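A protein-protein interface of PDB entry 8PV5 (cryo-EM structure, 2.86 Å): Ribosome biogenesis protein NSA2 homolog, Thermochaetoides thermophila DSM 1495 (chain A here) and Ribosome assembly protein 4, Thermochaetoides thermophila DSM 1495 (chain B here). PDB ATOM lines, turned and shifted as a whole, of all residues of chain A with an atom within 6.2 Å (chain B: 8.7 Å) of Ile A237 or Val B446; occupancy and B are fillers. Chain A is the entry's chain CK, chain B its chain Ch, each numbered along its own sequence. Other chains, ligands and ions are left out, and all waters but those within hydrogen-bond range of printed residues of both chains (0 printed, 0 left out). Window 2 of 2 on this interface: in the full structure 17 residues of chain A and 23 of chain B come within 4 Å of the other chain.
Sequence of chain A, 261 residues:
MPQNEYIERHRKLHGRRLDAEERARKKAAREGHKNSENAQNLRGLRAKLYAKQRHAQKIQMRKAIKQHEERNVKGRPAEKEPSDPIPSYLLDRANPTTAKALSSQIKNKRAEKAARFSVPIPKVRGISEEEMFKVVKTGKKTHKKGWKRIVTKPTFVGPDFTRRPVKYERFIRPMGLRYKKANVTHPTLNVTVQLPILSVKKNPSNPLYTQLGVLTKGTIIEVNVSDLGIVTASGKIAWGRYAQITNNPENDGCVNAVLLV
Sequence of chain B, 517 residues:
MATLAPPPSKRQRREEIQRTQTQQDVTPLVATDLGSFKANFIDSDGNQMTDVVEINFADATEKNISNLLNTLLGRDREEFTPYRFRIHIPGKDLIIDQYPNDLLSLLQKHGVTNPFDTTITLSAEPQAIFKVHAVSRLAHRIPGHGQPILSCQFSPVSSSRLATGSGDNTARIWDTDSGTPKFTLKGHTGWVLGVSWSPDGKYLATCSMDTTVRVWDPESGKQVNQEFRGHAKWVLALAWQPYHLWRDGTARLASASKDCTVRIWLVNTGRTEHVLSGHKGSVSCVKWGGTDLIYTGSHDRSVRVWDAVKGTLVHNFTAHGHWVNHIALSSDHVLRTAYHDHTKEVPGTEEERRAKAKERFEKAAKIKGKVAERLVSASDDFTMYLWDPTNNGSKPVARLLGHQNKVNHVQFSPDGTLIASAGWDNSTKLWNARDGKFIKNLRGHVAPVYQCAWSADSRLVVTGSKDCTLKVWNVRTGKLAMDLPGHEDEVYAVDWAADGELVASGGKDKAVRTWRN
The backbone carbonyl oxygen (O) of Val B446 sits close to the side-chain amide oxygen (OD1) of Asn B426 (3.4 Å). A ring nitrogen (ND1) of His B445 is in hydrogen-bond range of the side-chain carboxylate (OD2) of Asp B467, at 3.1 Å. The side-chain carboxylate (OD2) of Asp B467 lies within hydrogen-bond range of the backbone NH (N) of Val B446 (3.3 Å). The backbone NH (N) of Asp B467 lies close to the side-chain hydroxyl (OG) of Ser B465 (3.5 Å). The side-chain hydroxyl of Thr B469 lies within hydrogen-bond range of the side-chain carboxylate of Asp B467 (2.7 Å).
CA of Gly A229 touches CG2 of Val B446 (3.7 Å). Val B446 touches Val A231 (CG2 to CG2, 3.8 Å). CG2 of Val A231 touches O of Asp B467 (3.4 Å). Val A231 touches Thr B469. Ile A237 touches Val B446.
Printed residues of chain B within 4 Å of Ile A237: Val B446. Of the printed residues of chain A, Val B446 touches Gly A229, Val A231 and Ile A237. Of chain B, only Val B446 (3.7 Å) comes within 4 Å of Gly A229. Of the printed residues of chain A, Asp B467 touches Val A231. Of the printed residues of chain A, Thr B469 touches Val A231 (3.7 Å). Of the printed residues of chain B, Val A231 touches Val B446, Asp B467 and Thr B469. Trp B473 touches none of the printed residues of chain A. Cys B468 touches none of the printed residues of chain A. The nearest printed residue of chain B that does not touch Ile A237 is Gly B444 (5.0 Å). The nearest printed residue of chain A that does not touch Val B446 is Ile A230 (4.4 Å).
Of the 13 printed residues of chain A, 3 touch a printed residue of chain B. Hydrophobic or aromatic side chains of chain A within 4 Å of the printed part of chain B: Val A231 and Ile A237. Hydrophobic or aromatic side chains of chain B within 4 Å of the printed part of chain A: Val B446. Among the printed residues, no Asp or Glu carboxylate lies within 4 Å of a Lys or Arg side-chain nitrogen of the other chain.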
ATOM      1  N   SER A 226     -30.710 -17.517  26.689  1.00  0.00           N
ATOM      2  CA  SER A 226     -29.493 -16.866  27.168  1.00  0.00           C
ATOM      3  C   SER A 226     -28.733 -16.191  26.034  1.00  0.00           C
ATOM      4  O   SER A 226     -28.149 -15.118  26.220  1.00  0.00           O
ATOM      5  CB  SER A 226     -28.598 -17.889  27.867  1.00  0.00           C
ATOM      6  OG  SER A 226     -29.245 -18.449  28.992  1.00  0.00           O
ATOM      7  N   ASP A 227     -28.725 -16.811  24.852  1.00  0.00           N
ATOM      8  CA  ASP A 227     -27.962 -16.266  23.734  1.00  0.00           C
ATOM      9  C   ASP A 227     -28.623 -15.027  23.147  1.00  0.00           C
ATOM     10  O   ASP A 227     -27.945 -14.197  22.532  1.00  0.00           O
ATOM     11  CB  ASP A 227     -27.782 -17.333  22.656  1.00  0.00           C
ATOM     12  CG  ASP A 227     -26.946 -18.503  23.131  1.00  0.00           C
ATOM     13  OD1 ASP A 227     -26.365 -18.410  24.233  1.00  0.00           O
ATOM     14  OD2 ASP A 227     -26.870 -19.516  22.404  1.00  0.00           O
ATOM     15  N   LEU A 228     -29.937 -14.882  23.319  1.00  0.00           N
ATOM     16  CA  LEU A 228     -30.641 -13.716  22.805  1.00  0.00           C
ATOM     17  C   LEU A 228     -30.388 -12.457  23.621  1.00  0.00           C
ATOM     18  O   LEU A 228     -30.620 -11.355  23.113  1.00  0.00           O
ATOM     19  CB  LEU A 228     -32.142 -13.996  22.743  1.00  0.00           C
ATOM     20  CG  LEU A 228     -32.547 -15.006  21.673  1.00  0.00           C
ATOM     21  CD1 LEU A 228     -34.008 -15.358  21.804  1.00  0.00           C
ATOM     22  CD2 LEU A 228     -32.261 -14.442  20.297  1.00  0.00           C
ATOM     23  N   GLY A 229     -29.924 -12.590  24.862  1.00  0.00           N
ATOM     24  CA  GLY A 229     -29.586 -11.440  25.674  1.00  0.00           C
ATOM     25  C   GLY A 229     -30.777 -10.611  26.104  1.00  0.00           C
ATOM     26  O   GLY A 229     -30.908  -9.450  25.709  1.00  0.00           O
ATOM     27  N   ILE A 230     -31.650 -11.195  26.917  1.00  0.00           N
ATOM     28  CA  ILE A 230     -32.855 -10.528  27.392  1.00  0.00           C
ATOM     29  C   ILE A 230     -32.654 -10.169  28.856  1.00  0.00           C
ATOM     30  O   ILE A 230     -32.352 -11.039  29.682  1.00  0.00           O
ATOM     31  CB  ILE A 230     -34.098 -11.409  27.199  1.00  0.00           C
ATOM     32  CG1 ILE A 230     -34.253 -11.784  25.725  1.00  0.00           C
ATOM     33  CG2 ILE A 230     -35.338 -10.698  27.710  1.00  0.00           C
ATOM     34  CD1 ILE A 230     -35.411 -12.708  25.446  1.00  0.00           C
ATOM     35  N   VAL A 231     -32.814  -8.889  29.178  1.00  0.00           N
ATOM     36  CA  VAL A 231     -32.672  -8.384  30.537  1.00  0.00           C
ATOM     37  C   VAL A 231     -34.009  -7.812  30.979  1.00  0.00           C
ATOM     38  O   VAL A 231     -34.629  -7.026  30.254  1.00  0.00           O
ATOM     39  CB  VAL A 231     -31.561  -7.320  30.637  1.00  0.00           C
ATOM     40  CG1 VAL A 231     -31.343  -6.914  32.084  1.00  0.00           C
ATOM     41  CG2 VAL A 231     -30.271  -7.839  30.030  1.00  0.00           C
ATOM     42  N   THR A 232     -34.454  -8.210  32.166  1.00  0.00           N
ATOM     43  CA  THR A 232     -35.716  -7.732  32.704  1.00  0.00           C
ATOM     44  C   THR A 232     -35.572  -6.301  33.222  1.00  0.00           C
ATOM     45  O   THR A 232     -34.492  -5.705  33.201  1.00  0.00           O
ATOM     46  CB  THR A 232     -36.207  -8.656  33.816  1.00  0.00           C
ATOM     47  OG1 THR A 232     -35.381  -8.492  34.974  1.00  0.00           O
ATOM     48  CG2 THR A 232     -36.147 -10.104  33.364  1.00  0.00           C
ATOM     49  N   GLY A 235     -33.145  -5.764  36.114  1.00  0.00           N
ATOM     50  CA  GLY A 235     -31.757  -6.084  35.860  1.00  0.00           C
ATOM     51  C   GLY A 235     -31.428  -7.557  35.852  1.00  0.00           C
ATOM     52  O   GLY A 235     -30.270  -7.914  35.610  1.00  0.00           O
ATOM     53  N   LYS A 236     -32.403  -8.421  36.116  1.00  0.00           N
ATOM     54  CA  LYS A 236     -32.180  -9.855  36.065  1.00  0.00           C
ATOM     55  C   LYS A 236     -32.135 -10.336  34.619  1.00  0.00           C
ATOM     56  O   LYS A 236     -32.723  -9.734  33.717  1.00  0.00           O
ATOM     57  CB  LYS A 236     -33.274 -10.591  36.837  1.00  0.00           C
ATOM     58  CG  LYS A 236     -33.261 -10.307  38.327  1.00  0.00           C
ATOM     59  CD  LYS A 236     -34.400 -11.012  39.036  1.00  0.00           C
ATOM     60  CE  LYS A 236     -34.317 -10.802  40.535  1.00  0.00           C
ATOM     61  NZ  LYS A 236     -34.497  -9.371  40.899  1.00  0.00           N
ATOM     62  N   ILE A 237     -31.421 -11.433  34.404  1.00  0.00           N
ATOM     63  CA  ILE A 237     -31.253 -12.001  33.072  1.00  0.00           C
ATOM     64  C   ILE A 237     -32.337 -13.048  32.853  1.00  0.00           C
ATOM     65  O   ILE A 237     -32.430 -14.024  33.603  1.00  0.00           O
ATOM     66  CB  ILE A 237     -29.857 -12.613  32.898  1.00  0.00           C
ATOM     67  CG1 ILE A 237     -28.775 -11.609  33.301  1.00  0.00           C
ATOM     68  CG2 ILE A 237     -29.656 -13.072  31.466  1.00  0.00           C
ATOM     69  CD1 ILE A 237     -28.794 -10.333  32.499  1.00  0.00           C
ATOM     70  N   ALA A 238     -33.154 -12.845  31.825  1.00  0.00           N
ATOM     71  CA  ALA A 238     -34.182 -13.811  31.460  1.00  0.00           C
ATOM     72  C   ALA A 238     -33.553 -14.890  30.590  1.00  0.00           C
ATOM     73  O   ALA A 238     -33.180 -14.632  29.441  1.00  0.00           O
ATOM     74  CB  ALA A 238     -35.330 -13.120  30.731  1.00  0.00           C
ATOM     75  N   TRP A 239     -33.426 -16.100  31.133  1.00  0.00           N
ATOM     76  CA  TRP A 239     -32.841 -17.209  30.396  1.00  0.00           C
ATOM     77  C   TRP A 239     -33.828 -18.325  30.088  1.00  0.00           C
ATOM     78  O   TRP A 239     -33.405 -19.390  29.632  1.00  0.00           O
ATOM     79  CB  TRP A 239     -31.638 -17.783  31.158  1.00  0.00           C
ATOM     80  CG  TRP A 239     -31.971 -18.487  32.436  1.00  0.00           C
ATOM     81  CD1 TRP A 239     -32.284 -17.911  33.630  1.00  0.00           C
ATOM     82  CD2 TRP A 239     -31.990 -19.902  32.654  1.00  0.00           C
ATOM     83  NE1 TRP A 239     -32.512 -18.879  34.576  1.00  0.00           N
ATOM     84  CE2 TRP A 239     -32.337 -20.110  34.002  1.00  0.00           C
ATOM     85  CE3 TRP A 239     -31.755 -21.013  31.840  1.00  0.00           C
ATOM     86  CZ2 TRP A 239     -32.454 -21.382  34.552  1.00  0.00           C
ATOM     87  CZ3 TRP A 239     -31.873 -22.274  32.387  1.00  0.00           C
ATOM     88  CH2 TRP A 239     -32.221 -22.449  33.730  1.00  0.00           C
ATOM     89  N   GLY A 240     -35.118 -18.115  30.321  1.00  0.00           N
ATOM     90  CA  GLY A 240     -36.117 -19.090  29.937  1.00  0.00           C
ATOM     91  C   GLY A 240     -37.421 -18.434  29.541  1.00  0.00           C
ATOM     92  O   GLY A 240     -37.992 -17.667  30.320  1.00  0.00           O
ATOM     93  N   TRP B 424     -17.698  -7.436  20.815  1.00  0.00           N
ATOM     94  CA  TRP B 424     -18.936  -8.090  20.417  1.00  0.00           C
ATOM     95  C   TRP B 424     -19.074  -9.481  21.013  1.00  0.00           C
ATOM     96  O   TRP B 424     -20.083 -10.149  20.770  1.00  0.00           O
ATOM     97  CB  TRP B 424     -19.028  -8.164  18.891  1.00  0.00           C
ATOM     98  CG  TRP B 424     -19.351  -6.854  18.233  1.00  0.00           C
ATOM     99  CD1 TRP B 424     -18.669  -5.682  18.359  1.00  0.00           C
ATOM    100  CD2 TRP B 424     -20.432  -6.594  17.334  1.00  0.00           C
ATOM    101  NE1 TRP B 424     -19.261  -4.705  17.600  1.00  0.00           N
ATOM    102  CE2 TRP B 424     -20.347  -5.239  16.959  1.00  0.00           C
ATOM    103  CE3 TRP B 424     -21.468  -7.373  16.810  1.00  0.00           C
ATOM    104  CZ2 TRP B 424     -21.255  -4.647  16.088  1.00  0.00           C
ATOM    105  CZ3 TRP B 424     -22.369  -6.783  15.945  1.00  0.00           C
ATOM    106  CH2 TRP B 424     -22.257  -5.434  15.593  1.00  0.00           C
ATOM    107  N   ASP B 425     -18.082  -9.928  21.783  1.00  0.00           N
ATOM    108  CA  ASP B 425     -18.141 -11.185  22.514  1.00  0.00           C
ATOM    109  C   ASP B 425     -18.648 -10.990  23.936  1.00  0.00           C
ATOM    110  O   ASP B 425     -18.180 -11.676  24.852  1.00  0.00           O
ATOM    111  CB  ASP B 425     -16.768 -11.857  22.533  1.00  0.00           C
ATOM    112  CG  ASP B 425     -15.670 -10.918  22.972  1.00  0.00           C
ATOM    113  OD1 ASP B 425     -15.928  -9.703  23.074  1.00  0.00           O
ATOM    114  OD2 ASP B 425     -14.546 -11.397  23.222  1.00  0.00           O
ATOM    115  N   ASN B 426     -19.547 -10.022  24.134  1.00  0.00           N
ATOM    116  CA  ASN B 426     -20.246  -9.734  25.383  1.00  0.00           C
ATOM    117  C   ASN B 426     -19.311  -9.254  26.486  1.00  0.00           C
ATOM    118  O   ASN B 426     -19.690  -9.265  27.661  1.00  0.00           O
ATOM    119  CB  ASN B 426     -21.036 -10.951  25.886  1.00  0.00           C
ATOM    120  CG  ASN B 426     -22.123 -11.379  24.929  1.00  0.00           C
ATOM    121  OD1 ASN B 426     -22.756 -10.554  24.287  1.00  0.00           O
ATOM    122  ND2 ASN B 426     -22.353 -12.681  24.841  1.00  0.00           N
ATOM    123  N   SER B 427     -18.099  -8.820  26.149  1.00  0.00           N
ATOM    124  CA  SER B 427     -17.061  -8.638  27.150  1.00  0.00           C
ATOM    125  C   SER B 427     -16.366  -7.291  27.009  1.00  0.00           C
ATOM    126  O   SER B 427     -16.128  -6.784  25.907  1.00  0.00           O
ATOM    127  CB  SER B 427     -16.017  -9.759  27.074  1.00  0.00           C
ATOM    128  OG  SER B 427     -15.158  -9.575  25.965  1.00  0.00           O
ATOM    129  N   LEU B 442     -14.157  -8.204  32.209  1.00  0.00           N
ATOM    130  CA  LEU B 442     -15.391  -7.775  32.849  1.00  0.00           C
ATOM    131  C   LEU B 442     -16.557  -8.460  32.154  1.00  0.00           C
ATOM    132  O   LEU B 442     -16.888  -8.123  31.013  1.00  0.00           O
ATOM    133  CB  LEU B 442     -15.535  -6.254  32.784  1.00  0.00           C
ATOM    134  CG  LEU B 442     -14.309  -5.476  33.271  1.00  0.00           C
ATOM    135  CD1 LEU B 442     -14.436  -4.003  32.932  1.00  0.00           C
ATOM    136  CD2 LEU B 442     -14.099  -5.667  34.762  1.00  0.00           C
ATOM    137  N   ARG B 443     -17.183  -9.414  32.844  1.00  0.00           N
ATOM    138  CA  ARG B 443     -18.139 -10.335  32.235  1.00  0.00           C
ATOM    139  C   ARG B 443     -19.493 -10.197  32.936  1.00  0.00           C
ATOM    140  O   ARG B 443     -19.776 -10.881  33.920  1.00  0.00           O
ATOM    141  CB  ARG B 443     -17.617 -11.771  32.302  1.00  0.00           C
ATOM    142  CG  ARG B 443     -18.468 -12.790  31.572  1.00  0.00           C
ATOM    143  CD  ARG B 443     -18.073 -14.199  31.969  1.00  0.00           C
ATOM    144  NE  ARG B 443     -18.958 -15.201  31.390  1.00  0.00           N
ATOM    145  CZ  ARG B 443     -18.808 -16.509  31.546  1.00  0.00           C
ATOM    146  NH1 ARG B 443     -17.815 -17.010  32.261  1.00  0.00           N
ATOM    147  NH2 ARG B 443     -19.676 -17.334  30.968  1.00  0.00           N
ATOM    148  N   GLY B 444     -20.327  -9.290  32.432  1.00  0.00           N
ATOM    149  CA  GLY B 444     -21.679  -9.168  32.937  1.00  0.00           C
ATOM    150  C   GLY B 444     -22.734  -8.971  31.870  1.00  0.00           C
ATOM    151  O   GLY B 444     -23.928  -9.115  32.144  1.00  0.00           O
ATOM    152  N   HIS B 445     -22.313  -8.658  30.649  1.00  0.00           N
ATOM    153  CA  HIS B 445     -23.230  -8.309  29.571  1.00  0.00           C
ATOM    154  C   HIS B 445     -23.642  -9.566  28.818  1.00  0.00           C
ATOM    155  O   HIS B 445     -22.870 -10.525  28.730  1.00  0.00           O
ATOM    156  CB  HIS B 445     -22.592  -7.304  28.614  1.00  0.00           C
ATOM    157  CG  HIS B 445     -22.626  -5.890  29.107  1.00  0.00           C
ATOM    158  ND1 HIS B 445     -23.801  -5.197  29.302  1.00  0.00           N
ATOM    159  CD2 HIS B 445     -21.628  -5.036  29.430  1.00  0.00           C
ATOM    160  CE1 HIS B 445     -23.525  -3.979  29.733  1.00  0.00           C
ATOM    161  NE2 HIS B 445     -22.214  -3.855  29.818  1.00  0.00           N
ATOM    162  N   VAL B 446     -24.864  -9.555  28.281  1.00  0.00           N
ATOM    163  CA  VAL B 446     -25.379 -10.729  27.581  1.00  0.00           C
ATOM    164  C   VAL B 446     -25.584 -10.428  26.100  1.00  0.00           C
ATOM    165  O   VAL B 446     -25.904 -11.321  25.307  1.00  0.00           O
ATOM    166  CB  VAL B 446     -26.672 -11.220  28.255  1.00  0.00           C
ATOM    167  CG1 VAL B 446     -26.353 -11.851  29.599  1.00  0.00           C
ATOM    168  CG2 VAL B 446     -27.628 -10.066  28.450  1.00  0.00           C
ATOM    169  N   ALA B 447     -25.411  -9.175  25.709  1.00  0.00           N
ATOM    170  CA  ALA B 447     -25.431  -8.714  24.332  1.00  0.00           C
ATOM    171  C   ALA B 447     -24.177  -7.888  24.061  1.00  0.00           C
ATOM    172  O   ALA B 447     -23.503  -7.448  24.999  1.00  0.00           O
ATOM    173  CB  ALA B 447     -26.699  -7.895  24.068  1.00  0.00           C
ATOM    174  N   PRO B 448     -23.783  -7.710  22.760  1.00  0.00           N
ATOM    175  CA  PRO B 448     -22.537  -6.988  22.445  1.00  0.00           C
ATOM    176  C   PRO B 448     -22.405  -5.597  23.051  1.00  0.00           C
ATOM    177  O   PRO B 448     -23.337  -4.789  23.004  1.00  0.00           O
ATOM    178  CB  PRO B 448     -22.576  -6.901  20.918  1.00  0.00           C
ATOM    179  CG  PRO B 448     -23.259  -8.134  20.507  1.00  0.00           C
ATOM    180  CD  PRO B 448     -24.264  -8.465  21.584  1.00  0.00           C
ATOM    181  N   VAL B 449     -21.236  -5.322  23.623  1.00  0.00           N
ATOM    182  CA  VAL B 449     -20.965  -4.073  24.322  1.00  0.00           C
ATOM    183  C   VAL B 449     -20.591  -3.027  23.284  1.00  0.00           C
ATOM    184  O   VAL B 449     -19.569  -3.156  22.601  1.00  0.00           O
ATOM    185  CB  VAL B 449     -19.846  -4.244  25.360  1.00  0.00           C
ATOM    186  CG1 VAL B 449     -19.730  -3.002  26.221  1.00  0.00           C
ATOM    187  CG2 VAL B 449     -20.099  -5.472  26.212  1.00  0.00           C
ATOM    188  N   SER B 465     -24.411  -1.369  26.525  1.00  0.00           N
ATOM    189  CA  SER B 465     -24.459  -2.482  25.588  1.00  0.00           C
ATOM    190  C   SER B 465     -25.810  -2.581  24.892  1.00  0.00           C
ATOM    191  O   SER B 465     -26.731  -1.797  25.131  1.00  0.00           O
ATOM    192  CB  SER B 465     -24.149  -3.806  26.294  1.00  0.00           C
ATOM    193  OG  SER B 465     -24.388  -4.907  25.436  1.00  0.00           O
ATOM    194  N   LYS B 466     -25.901  -3.581  24.012  1.00  0.00           N
ATOM    195  CA  LYS B 466     -27.108  -3.880  23.255  1.00  0.00           C
ATOM    196  C   LYS B 466     -28.195  -4.507  24.126  1.00  0.00           C
ATOM    197  O   LYS B 466     -29.374  -4.464  23.754  1.00  0.00           O
ATOM    198  CB  LYS B 466     -26.730  -4.793  22.078  1.00  0.00           C
ATOM    199  CG  LYS B 466     -27.851  -5.191  21.131  1.00  0.00           C
ATOM    200  CD  LYS B 466     -27.359  -6.122  20.039  1.00  0.00           C
ATOM    201  CE  LYS B 466     -28.485  -6.469  19.080  1.00  0.00           C
ATOM    202  NZ  LYS B 466     -28.065  -7.462  18.055  1.00  0.00           N
ATOM    203  N   ASP B 467     -27.845  -5.017  25.308  1.00  0.00           N
ATOM    204  CA  ASP B 467     -28.806  -5.646  26.206  1.00  0.00           C
ATOM    205  C   ASP B 467     -29.627  -4.646  27.011  1.00  0.00           C
ATOM    206  O   ASP B 467     -30.172  -5.028  28.053  1.00  0.00           O
ATOM    207  CB  ASP B 467     -28.100  -6.627  27.152  1.00  0.00           C
ATOM    208  CG  ASP B 467     -27.041  -5.968  28.033  1.00  0.00           C
ATOM    209  OD1 ASP B 467     -26.819  -4.744  27.945  1.00  0.00           O
ATOM    210  OD2 ASP B 467     -26.421  -6.695  28.836  1.00  0.00           O
ATOM    211  N   CYS B 468     -29.688  -3.390  26.569  1.00  0.00           N
ATOM    212  CA  CYS B 468     -30.443  -2.268  27.117  1.00  0.00           C
ATOM    213  C   CYS B 468     -29.897  -1.818  28.466  1.00  0.00           C
ATOM    214  O   CYS B 468     -30.592  -1.084  29.175  1.00  0.00           O
ATOM    215  CB  CYS B 468     -31.944  -2.568  27.265  1.00  0.00           C
ATOM    216  SG  CYS B 468     -32.681  -3.422  25.854  1.00  0.00           S
ATOM    217  N   THR B 469     -28.687  -2.221  28.850  1.00  0.00           N
ATOM    218  CA  THR B 469     -28.151  -1.900  30.162  1.00  0.00           C
ATOM    219  C   THR B 469     -26.815  -1.174  30.061  1.00  0.00           C
ATOM    220  O   THR B 469     -26.047  -1.327  29.096  1.00  0.00           O
ATOM    221  CB  THR B 469     -27.963  -3.156  31.033  1.00  0.00           C
ATOM    222  OG1 THR B 469     -26.842  -3.911  30.560  1.00  0.00           O
ATOM    223  CG2 THR B 469     -29.206  -4.026  31.036  1.00  0.00           C
ATOM    224  N   LYS B 471     -23.389  -0.705  32.659  1.00  0.00           N
ATOM    225  CA  LYS B 471     -22.753  -1.340  33.801  1.00  0.00           C
ATOM    226  C   LYS B 471     -21.507  -0.568  34.195  1.00  0.00           C
ATOM    227  O   LYS B 471     -20.640  -0.302  33.359  1.00  0.00           O
ATOM    228  CB  LYS B 471     -22.404  -2.802  33.505  1.00  0.00           C
ATOM    229  CG  LYS B 471     -23.622  -3.684  33.288  1.00  0.00           C
ATOM    230  CD  LYS B 471     -23.278  -5.153  33.317  1.00  0.00           C
ATOM    231  CE  LYS B 471     -24.448  -5.974  32.825  1.00  0.00           C
ATOM    232  NZ  LYS B 471     -25.714  -5.573  33.488  1.00  0.00           N
ATOM    233  N   TRP B 473     -18.146  -0.640  36.278  1.00  0.00           N
ATOM    234  CA  TRP B 473     -17.184  -1.628  36.734  1.00  0.00           C
ATOM    235  C   TRP B 473     -16.090  -0.926  37.518  1.00  0.00           C
ATOM    236  O   TRP B 473     -15.516   0.058  37.038  1.00  0.00           O
ATOM    237  CB  TRP B 473     -16.564  -2.379  35.555  1.00  0.00           C
ATOM    238  CG  TRP B 473     -17.555  -2.964  34.614  1.00  0.00           C
ATOM    239  CD1 TRP B 473     -18.143  -2.344  33.553  1.00  0.00           C
ATOM    240  CD2 TRP B 473     -18.069  -4.296  34.638  1.00  0.00           C
ATOM    241  NE1 TRP B 473     -19.000  -3.208  32.919  1.00  0.00           N
ATOM    242  CE2 TRP B 473     -18.971  -4.414  33.567  1.00  0.00           C
ATOM    243  CE3 TRP B 473     -17.857  -5.400  35.467  1.00  0.00           C
ATOM    244  CZ2 TRP B 473     -19.660  -5.591  33.302  1.00  0.00           C
ATOM    245  CZ3 TRP B 473     -18.541  -6.565  35.203  1.00  0.00           C
ATOM    246  CH2 TRP B 473     -19.430  -6.653  34.131  1.00  0.00           C
ATOM    247  N   LEU B 480     -18.297  -5.832  39.079  1.00  0.00           N
ATOM    248  CA  LEU B 480     -19.454  -5.031  38.703  1.00  0.00           C
ATOM    249  C   LEU B 480     -19.916  -4.202  39.894  1.00  0.00           C
ATOM    250  O   LEU B 480     -20.609  -4.710  40.783  1.00  0.00           O
ATOM    251  CB  LEU B 480     -20.575  -5.938  38.207  1.00  0.00           C
ATOM    252  CG  LEU B 480     -21.864  -5.241  37.786  1.00  0.00           C
ATOM    253  CD1 LEU B 480     -21.550  -4.265  36.692  1.00  0.00           C
ATOM    254  CD2 LEU B 480     -22.891  -6.252  37.317  1.00  0.00           C
ATOM    255  N   ASP B 483     -25.165  -1.676  38.443  1.00  0.00           N
ATOM    256  CA  ASP B 483     -25.965  -2.044  37.286  1.00  0.00           C
ATOM    257  C   ASP B 483     -27.042  -0.990  37.056  1.00  0.00           C
ATOM    258  O   ASP B 483     -27.730  -0.571  37.990  1.00  0.00           O
ATOM    259  CB  ASP B 483     -26.611  -3.416  37.486  1.00  0.00           C
ATOM    260  CG  ASP B 483     -26.847  -4.144  36.181  1.00  0.00           C
ATOM    261  OD1 ASP B 483     -26.937  -3.474  35.133  1.00  0.00           O
ATOM    262  OD2 ASP B 483     -26.944  -5.387  36.205  1.00  0.00           O
